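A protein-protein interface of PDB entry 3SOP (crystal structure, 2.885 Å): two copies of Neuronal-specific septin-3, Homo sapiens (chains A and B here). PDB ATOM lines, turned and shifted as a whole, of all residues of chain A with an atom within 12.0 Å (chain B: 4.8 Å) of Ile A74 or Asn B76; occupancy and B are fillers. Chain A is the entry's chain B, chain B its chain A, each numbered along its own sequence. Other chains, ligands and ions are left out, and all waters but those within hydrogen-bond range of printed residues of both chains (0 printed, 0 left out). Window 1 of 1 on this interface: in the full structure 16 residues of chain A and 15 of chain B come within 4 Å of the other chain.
The side-chain amide nitrogen (ND2) of Asn B76 sits close to the backbone NH (N) of Asp B72 (3.0 Å). O of Gln B73 is in hydrogen-bond range of ND2 of Asn B76 (3.0 Å). N of Asp A72 sits close to ND2 of Asn A76, at 3.2 Å. ND2 of Asn A76 lies within hydrogen-bond range of O of Gln A73 (3.2 Å).
Asp A72 touches Pro B128, but with the chains exchanged Pro A128 does not touch Asp B72 (5.1 Å). Asn A75 touches its own counterpart, Asn B75. Glu A77 touches Ile B74, but with the chains exchanged Ile A74 does not touch Glu B77 (4.6 Å). Glu A77 touches Asn B75, but with the chains exchanged Asn A75 does not touch Glu B77 (5.8 Å). Positions printed for both chains: 72, 73, 74, 75, 76, 77, 78, 79, 128 and 129. Of the 10 pairs that touch across the chains among the printed residues, 5 have their exchanged pair printed and touching as well.
Hydrophobic or aromatic side chains of chain B that line the printed part of chain A: Ile B74, Pro B128 and Leu B129. Along chain B the printed residues that touch a printed residue of chain A span positions 74 to 129. Of the 17 printed residues of chain A, 6 touch a printed residue of chain B. Printed residues of chain A that touch a printed residue of chain B: Asp A72, Ile A74, Asn A75, Asn A76, Glu A77 and Leu A129. Among the printed residues, no Asp or Glu carboxylate lies within 4 Å of a Lys or Arg side-chain nitrogen of the other chain.
Ile A74 touches three residues of chain B. Printed residues of chain B within 4 Å of Asn A75: Ile B74 (3.99 Å) and Asn B75 (2.7 Å). Printed residues of chain B within 4 Å of Asn A76: Ile B74 (2.9 Å). Printed residues of chain B within 4 Å of Glu A77: Ile B74 and Asn B75. Of the printed residues of chain B, Leu A129 touches Ile B74 (3.9 Å). No residue of chain A comes within 4 Å of Asp B72. Of the printed residues of chain A, Ile B74 touches Asn A75, Asn A76, Glu A77 and Leu A129. Of chain A, only Ile A74 (3.2 Å) comes within 4 Å of Asn B76. No residue of chain A comes within 4 Å of Glu B77. No residue of chain A comes within 4 Å of Asn B78. Cys B79 touches none of the printed residues of chain A. Of chain A, only Asp A72 and Ile A74 come within 4 Å of Pro B128. The nearest residue of chain B that does not touch Ile A74 is Asn B75 (4.4 Å). The nearest printed residue of chain B that does not touch Asn A75 is Asn B76 (4.5 Å).
O of Asp A72 touches CD of Pro B128, at 3.7 Å. CD1 of Ile A74 touches C of Pro B128, 3.7 Å away. Ile A74 touches Leu B129 (CD1 to CA, 3.4 Å). Ile B74 touches Asn A75 (O to C, 3.99 Å). Ile B74 touches Glu A77 (CG2 to OE1, 2.8 Å). Asn B75 touches Glu A77 (CB to OE2, 3.8 Å). Ile B74 touches Leu A129.
The side-chain amide oxygen of Asn B75 lies within hydrogen-bond range of the side-chain amide nitrogen of Asn A75, at 2.7 Å. O of Ile B74 sits at hydrogen-bond distance from N of Asn A76 (2.9 Å). N of Asn B76 lies close to O of Ile A74, at 3.2 Å.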
ATOM      1  N   GLN A  10      -8.431 -15.282  17.668  1.00  0.00           N
ATOM      2  CA  GLN A  10      -7.925 -16.047  18.804  1.00  0.00           C
ATOM      3  C   GLN A  10      -6.431 -15.798  19.017  1.00  0.00           C
ATOM      4  O   GLN A  10      -5.715 -15.386  18.101  1.00  0.00           O
ATOM      5  CB  GLN A  10      -8.217 -17.543  18.651  1.00  0.00           C
ATOM      6  CG  GLN A  10      -7.504 -18.206  17.487  1.00  0.00           C
ATOM      7  CD  GLN A  10      -7.797 -19.688  17.402  1.00  0.00           C
ATOM      8  OE1 GLN A  10      -8.598 -20.213  18.173  1.00  0.00           O
ATOM      9  NE2 GLN A  10      -7.150 -20.372  16.464  1.00  0.00           N
ATOM     10  N   SER A  11      -5.978 -16.052  20.239  1.00  0.00           N
ATOM     11  CA  SER A  11      -4.617 -15.733  20.655  1.00  0.00           C
ATOM     12  C   SER A  11      -3.545 -16.555  19.937  1.00  0.00           C
ATOM     13  O   SER A  11      -3.767 -17.710  19.581  1.00  0.00           O
ATOM     14  CB  SER A  11      -4.485 -15.909  22.167  1.00  0.00           C
ATOM     15  OG  SER A  11      -3.186 -15.565  22.600  1.00  0.00           O
ATOM     16  N   GLY A  69      -6.777 -12.329  23.323  1.00  0.00           N
ATOM     17  CA  GLY A  69      -7.497 -13.589  23.235  1.00  0.00           C
ATOM     18  C   GLY A  69      -8.761 -13.568  22.399  1.00  0.00           C
ATOM     19  O   GLY A  69      -8.867 -12.813  21.429  1.00  0.00           O
ATOM     20  N   PHE A  70      -9.719 -14.409  22.782  1.00  0.00           N
ATOM     21  CA  PHE A  70     -11.009 -14.507  22.104  1.00  0.00           C
ATOM     22  C   PHE A  70     -11.750 -15.761  22.557  1.00  0.00           C
ATOM     23  O   PHE A  70     -11.161 -16.837  22.668  1.00  0.00           O
ATOM     24  CB  PHE A  70     -10.831 -14.532  20.585  1.00  0.00           C
ATOM     25  N   ASP A  72      -9.821 -19.832  22.849  1.00  0.00           N
ATOM     26  CA  ASP A  72      -8.618 -19.467  23.584  1.00  0.00           C
ATOM     27  C   ASP A  72      -8.778 -19.757  25.078  1.00  0.00           C
ATOM     28  O   ASP A  72      -7.809 -19.701  25.838  1.00  0.00           O
ATOM     29  CB  ASP A  72      -8.273 -17.992  23.349  1.00  0.00           C
ATOM     30  N   GLN A  73     -10.005 -20.075  25.489  1.00  0.00           N
ATOM     31  CA  GLN A  73     -10.302 -20.371  26.890  1.00  0.00           C
ATOM     32  C   GLN A  73     -11.214 -21.589  27.036  1.00  0.00           C
ATOM     33  O   GLN A  73     -11.798 -22.061  26.059  1.00  0.00           O
ATOM     34  CB  GLN A  73     -10.936 -19.159  27.581  1.00  0.00           C
ATOM     35  N   ILE A  74     -11.332 -22.087  28.264  1.00  0.00           N
ATOM     36  CA  ILE A  74     -12.180 -23.239  28.560  1.00  0.00           C
ATOM     37  C   ILE A  74     -13.586 -23.070  27.992  1.00  0.00           C
ATOM     38  O   ILE A  74     -14.019 -23.826  27.120  1.00  0.00           O
ATOM     39  CB  ILE A  74     -12.309 -23.463  30.080  1.00  0.00           C
ATOM     40  CG1 ILE A  74     -10.945 -23.348  30.767  1.00  0.00           C
ATOM     41  CG2 ILE A  74     -12.944 -24.818  30.366  1.00  0.00           C
ATOM     42  CD1 ILE A  74      -9.990 -24.467  30.418  1.00  0.00           C
ATOM     43  N   ASN A  75     -14.301 -22.081  28.514  1.00  0.00           N
ATOM     44  CA  ASN A  75     -15.630 -21.748  28.023  1.00  0.00           C
ATOM     45  C   ASN A  75     -15.653 -20.373  27.356  1.00  0.00           C
ATOM     46  O   ASN A  75     -15.437 -19.355  28.013  1.00  0.00           O
ATOM     47  CB  ASN A  75     -16.639 -21.797  29.167  1.00  0.00           C
ATOM     48  CG  ASN A  75     -17.948 -21.137  28.811  1.00  0.00           C
ATOM     49  OD1 ASN A  75     -18.135 -19.944  29.045  1.00  0.00           O
ATOM     50  ND2 ASN A  75     -18.862 -21.905  28.236  1.00  0.00           N
ATOM     51  N   ASN A  76     -15.918 -20.354  26.051  1.00  0.00           N
ATOM     52  CA  ASN A  76     -15.909 -19.120  25.268  1.00  0.00           C
ATOM     53  C   ASN A  76     -17.301 -18.666  24.838  1.00  0.00           C
ATOM     54  O   ASN A  76     -17.671 -18.782  23.671  1.00  0.00           O
ATOM     55  CB  ASN A  76     -15.021 -19.277  24.032  1.00  0.00           C
ATOM     56  CG  ASN A  76     -13.572 -19.538  24.385  1.00  0.00           C
ATOM     57  OD1 ASN A  76     -13.049 -18.986  25.351  1.00  0.00           O
ATOM     58  ND2 ASN A  76     -12.915 -20.386  23.601  1.00  0.00           N
ATOM     59  N   GLU A  77     -18.068 -18.146  25.788  1.00  0.00           N
ATOM     60  CA  GLU A  77     -19.404 -17.649  25.502  1.00  0.00           C
ATOM     61  C   GLU A  77     -19.368 -16.140  25.411  1.00  0.00           C
ATOM     62  O   GLU A  77     -18.689 -15.488  26.194  1.00  0.00           O
ATOM     63  CB  GLU A  77     -20.378 -18.060  26.604  1.00  0.00           C
ATOM     64  CG  GLU A  77     -20.446 -19.551  26.852  1.00  0.00           C
ATOM     65  CD  GLU A  77     -20.953 -20.321  25.649  1.00  0.00           C
ATOM     66  OE1 GLU A  77     -20.614 -19.948  24.507  1.00  0.00           O
ATOM     67  OE2 GLU A  77     -21.699 -21.302  25.845  1.00  0.00           O
ATOM     68  N   ASN A  78     -20.095 -15.582  24.454  1.00  0.00           N
ATOM     69  CA  ASN A  78     -20.184 -14.134  24.327  1.00  0.00           C
ATOM     70  C   ASN A  78     -18.827 -13.452  24.476  1.00  0.00           C
ATOM     71  O   ASN A  78     -18.747 -12.310  24.932  1.00  0.00           O
ATOM     72  CB  ASN A  78     -21.143 -13.571  25.376  1.00  0.00           C
ATOM     73  CG  ASN A  78     -22.458 -14.325  25.438  1.00  0.00           C
ATOM     74  OD1 ASN A  78     -22.651 -15.325  24.744  1.00  0.00           O
ATOM     75  ND2 ASN A  78     -23.366 -13.855  26.283  1.00  0.00           N
ATOM     76  N   CYS A  79     -17.765 -14.159  24.101  1.00  0.00           N
ATOM     77  CA  CYS A  79     -16.412 -13.623  24.193  1.00  0.00           C
ATOM     78  C   CYS A  79     -16.245 -12.441  23.246  1.00  0.00           C
ATOM     79  O   CYS A  79     -15.184 -11.824  23.178  1.00  0.00           O
ATOM     80  CB  CYS A  79     -15.386 -14.709  23.873  1.00  0.00           C
ATOM     81  SG  CYS A  79     -15.685 -15.542  22.304  1.00  0.00           S
ATOM     82  N   TRP A  80     -17.309 -12.135  22.513  1.00  0.00           N
ATOM     83  CA  TRP A  80     -17.331 -10.994  21.614  1.00  0.00           C
ATOM     84  C   TRP A  80     -17.879  -9.772  22.331  1.00  0.00           C
ATOM     85  O   TRP A  80     -17.587  -8.638  21.953  1.00  0.00           O
ATOM     86  CB  TRP A  80     -18.192 -11.307  20.395  1.00  0.00           C
ATOM     87  CG  TRP A  80     -19.445 -12.042  20.734  1.00  0.00           C
ATOM     88  CD1 TRP A  80     -20.609 -11.506  21.191  1.00  0.00           C
ATOM     89  CD2 TRP A  80     -19.660 -13.457  20.641  1.00  0.00           C
ATOM     90  NE1 TRP A  80     -21.542 -12.497  21.389  1.00  0.00           N
ATOM     91  CE2 TRP A  80     -20.985 -13.703  21.058  1.00  0.00           C
ATOM     92  CE3 TRP A  80     -18.863 -14.536  20.248  1.00  0.00           C
ATOM     93  CZ2 TRP A  80     -21.529 -14.988  21.093  1.00  0.00           C
ATOM     94  CZ3 TRP A  80     -19.407 -15.813  20.282  1.00  0.00           C
ATOM     95  CH2 TRP A  80     -20.727 -16.026  20.701  1.00  0.00           C
ATOM     96  N   ARG A 127     -14.124 -22.931  12.639  1.00  0.00           N
ATOM     97  CA  ARG A 127     -14.673 -23.274  13.946  1.00  0.00           C
ATOM     98  C   ARG A 127     -15.943 -22.476  14.238  1.00  0.00           C
ATOM     99  O   ARG A 127     -15.978 -21.263  14.038  1.00  0.00           O
ATOM    100  CB  ARG A 127     -13.630 -23.049  15.041  1.00  0.00           C
ATOM    101  CG  ARG A 127     -12.372 -23.892  14.873  1.00  0.00           C
ATOM    102  CD  ARG A 127     -11.315 -23.551  15.917  1.00  0.00           C
ATOM    103  NE  ARG A 127     -10.830 -22.178  15.790  1.00  0.00           N
ATOM    104  CZ  ARG A 127     -11.241 -21.167  16.547  1.00  0.00           C
ATOM    105  NH1 ARG A 127     -12.145 -21.371  17.496  1.00  0.00           N
ATOM    106  NH2 ARG A 127     -10.744 -19.951  16.360  1.00  0.00           N
ATOM    107  N   PRO A 128     -16.997 -23.164  14.704  1.00  0.00           N
ATOM    108  CA  PRO A 128     -18.299 -22.547  14.987  1.00  0.00           C
ATOM    109  C   PRO A 128     -18.194 -21.284  15.838  1.00  0.00           C
ATOM    110  O   PRO A 128     -19.006 -20.374  15.672  1.00  0.00           O
ATOM    111  CB  PRO A 128     -19.037 -23.643  15.755  1.00  0.00           C
ATOM    112  CG  PRO A 128     -18.472 -24.911  15.203  1.00  0.00           C
ATOM    113  CD  PRO A 128     -17.017 -24.619  14.931  1.00  0.00           C
ATOM    114  N   LEU A 129     -17.219 -21.234  16.741  1.00  0.00           N
ATOM    115  CA  LEU A 129     -16.997 -20.035  17.538  1.00  0.00           C
ATOM    116  C   LEU A 129     -16.548 -18.892  16.635  1.00  0.00           C
ATOM    117  O   LEU A 129     -17.034 -17.766  16.745  1.00  0.00           O
ATOM    118  CB  LEU A 129     -15.949 -20.284  18.623  1.00  0.00           C
ATOM    119  CG  LEU A 129     -15.525 -19.031  19.394  1.00  0.00           C
ATOM    120  CD1 LEU A 129     -16.714 -18.442  20.136  1.00  0.00           C
ATOM    121  CD2 LEU A 129     -14.379 -19.327  20.350  1.00  0.00           C
ATOM    122  N   ASP A 130     -15.610 -19.194  15.741  1.00  0.00           N
ATOM    123  CA  ASP A 130     -15.132 -18.226  14.763  1.00  0.00           C
ATOM    124  C   ASP A 130     -16.301 -17.618  13.992  1.00  0.00           C
ATOM    125  O   ASP A 130     -16.350 -16.407  13.787  1.00  0.00           O
ATOM    126  CB  ASP A 130     -14.135 -18.882  13.796  1.00  0.00           C
ATOM    127  CG  ASP A 130     -12.689 -18.696  14.229  1.00  0.00           C
ATOM    128  OD1 ASP A 130     -12.475 -18.148  15.327  1.00  0.00           O
ATOM    129  OD2 ASP A 130     -11.771 -19.097  13.480  1.00  0.00           O
ATOM    130  N   ASP B  72     -11.975 -26.192  21.022  1.00  0.00           N
ATOM    131  CA  ASP B  72     -12.462 -26.521  19.688  1.00  0.00           C
ATOM    132  C   ASP B  72     -13.976 -26.420  19.593  1.00  0.00           C
ATOM    133  O   ASP B  72     -14.600 -27.070  18.754  1.00  0.00           O
ATOM    134  CB  ASP B  72     -12.010 -27.923  19.287  1.00  0.00           C
ATOM    135  N   GLN B  73     -14.562 -25.603  20.460  1.00  0.00           N
ATOM    136  CA  GLN B  73     -16.002 -25.391  20.454  1.00  0.00           C
ATOM    137  C   GLN B  73     -16.347 -24.211  21.343  1.00  0.00           C
ATOM    138  O   GLN B  73     -15.584 -23.857  22.242  1.00  0.00           O
ATOM    139  CB  GLN B  73     -16.741 -26.647  20.922  1.00  0.00           C
ATOM    140  N   ILE B  74     -17.498 -23.599  21.089  1.00  0.00           N
ATOM    141  CA  ILE B  74     -17.898 -22.417  21.834  1.00  0.00           C
ATOM    142  C   ILE B  74     -17.869 -22.711  23.327  1.00  0.00           C
ATOM    143  O   ILE B  74     -17.464 -21.869  24.129  1.00  0.00           O
ATOM    144  CB  ILE B  74     -19.295 -21.929  21.422  1.00  0.00           C
ATOM    145  CG1 ILE B  74     -19.425 -21.929  19.899  1.00  0.00           C
ATOM    146  CG2 ILE B  74     -19.555 -20.538  21.969  1.00  0.00           C
ATOM    147  CD1 ILE B  74     -20.682 -21.255  19.389  1.00  0.00           C
ATOM    148  N   ASN B  75     -18.293 -23.915  23.693  1.00  0.00           N
ATOM    149  CA  ASN B  75     -18.210 -24.362  25.074  1.00  0.00           C
ATOM    150  C   ASN B  75     -17.459 -25.681  25.187  1.00  0.00           C
ATOM    151  O   ASN B  75     -17.877 -26.695  24.626  1.00  0.00           O
ATOM    152  CB  ASN B  75     -19.599 -24.493  25.694  1.00  0.00           C
ATOM    153  CG  ASN B  75     -19.543 -24.719  27.189  1.00  0.00           C
ATOM    154  OD1 ASN B  75     -18.490 -24.567  27.811  1.00  0.00           O
ATOM    155  ND2 ASN B  75     -20.676 -25.079  27.777  1.00  0.00           N
ATOM    156  N   ASN B  76     -16.345 -25.656  25.912  1.00  0.00           N
ATOM    157  CA  ASN B  76     -15.502 -26.833  26.073  1.00  0.00           C
ATOM    158  C   ASN B  76     -15.402 -27.268  27.525  1.00  0.00           C
ATOM    159  O   ASN B  76     -14.309 -27.348  28.085  1.00  0.00           O
ATOM    160  CB  ASN B  76     -14.106 -26.570  25.511  1.00  0.00           C
ATOM    161  CG  ASN B  76     -14.107 -26.406  24.007  1.00  0.00           C
ATOM    162  OD1 ASN B  76     -14.774 -27.153  23.293  1.00  0.00           O
ATOM    163  ND2 ASN B  76     -13.367 -25.418  23.518  1.00  0.00           N
ATOM    164  N   GLU B  77     -16.549 -27.547  28.130  1.00  0.00           N
ATOM    165  CA  GLU B  77     -16.590 -28.004  29.509  1.00  0.00           C
ATOM    166  C   GLU B  77     -16.579 -29.527  29.545  1.00  0.00           C
ATOM    167  O   GLU B  77     -17.444 -30.176  28.957  1.00  0.00           O
ATOM    168  CB  GLU B  77     -17.833 -27.459  30.213  1.00  0.00           C
ATOM    169  N   ASN B  78     -15.588 -30.091  30.228  1.00  0.00           N
ATOM    170  CA  ASN B  78     -15.446 -31.539  30.321  1.00  0.00           C
ATOM    171  C   ASN B  78     -15.328 -32.187  28.946  1.00  0.00           C
ATOM    172  O   ASN B  78     -15.986 -33.186  28.659  1.00  0.00           O
ATOM    173  CB  ASN B  78     -16.624 -32.144  31.082  1.00  0.00           C
ATOM    174  CG  ASN B  78     -16.885 -31.449  32.402  1.00  0.00           C
ATOM    175  OD1 ASN B  78     -15.961 -30.963  33.054  1.00  0.00           O
ATOM    176  ND2 ASN B  78     -18.150 -31.396  32.802  1.00  0.00           N
ATOM    177  N   CYS B  79     -14.485 -31.607  28.100  1.00  0.00           N
ATOM    178  CA  CYS B  79     -14.269 -32.125  26.756  1.00  0.00           C
ATOM    179  C   CYS B  79     -13.320 -33.322  26.772  1.00  0.00           C
ATOM    180  O   CYS B  79     -13.129 -33.986  25.753  1.00  0.00           O
ATOM    181  CB  CYS B  79     -13.709 -31.024  25.856  1.00  0.00           C
ATOM    182  SG  CYS B  79     -12.240 -30.213  26.526  1.00  0.00           S
ATOM    183  N   PRO B 128      -5.300 -22.347  28.851  1.00  0.00           N
ATOM    184  CA  PRO B 128      -5.807 -22.996  30.062  1.00  0.00           C
ATOM    185  C   PRO B 128      -6.394 -24.373  29.758  1.00  0.00           C
ATOM    186  O   PRO B 128      -6.210 -25.299  30.548  1.00  0.00           O
ATOM    187  CB  PRO B 128      -6.913 -22.046  30.526  1.00  0.00           C
ATOM    188  CG  PRO B 128      -6.511 -20.716  29.989  1.00  0.00           C
ATOM    189  CD  PRO B 128      -5.878 -21.007  28.659  1.00  0.00           C
ATOM    190  N   LEU B 129      -7.086 -24.502  28.630  1.00  0.00           N
ATOM    191  CA  LEU B 129      -7.717 -25.766  28.256  1.00  0.00           C
ATOM    192  C   LEU B 129      -6.687 -26.869  28.030  1.00  0.00           C
ATOM    193  O   LEU B 129      -6.873 -27.999  28.479  1.00  0.00           O
ATOM    194  CB  LEU B 129      -8.600 -25.587  27.016  1.00  0.00           C
ATOM    195  CG  LEU B 129      -9.416 -26.797  26.548  1.00  0.00           C
ATOM    196  CD1 LEU B 129     -10.710 -26.349  25.886  1.00  0.00           C
ATOM    197  CD2 LEU B 129      -8.610 -27.692  25.614  1.00  0.00           C
ATOM    198  N   GLU B 132      -5.347 -28.060  31.642  1.00  0.00           N
ATOM    199  CA  GLU B 132      -6.296 -28.897  32.367  1.00  0.00           C
ATOM    200  C   GLU B 132      -6.461 -30.253  31.700  1.00  0.00           C
ATOM    201  O   GLU B 132      -6.486 -31.286  32.369  1.00  0.00           O
ATOM    202  CB  GLU B 132      -7.656 -28.210  32.491  1.00  0.00           C
ATOM    203  CG  GLU B 132      -7.885 -27.523  33.826  1.00  0.00           C
ATOM    204  CD  GLU B 132      -9.360 -27.374  34.152  1.00  0.00           C
ATOM    205  OE1 GLU B 132      -9.698 -26.586  35.062  1.00  0.00           O
ATOM    206  OE2 GLU B 132     -10.182 -28.048  33.500  1.00  0.00           O
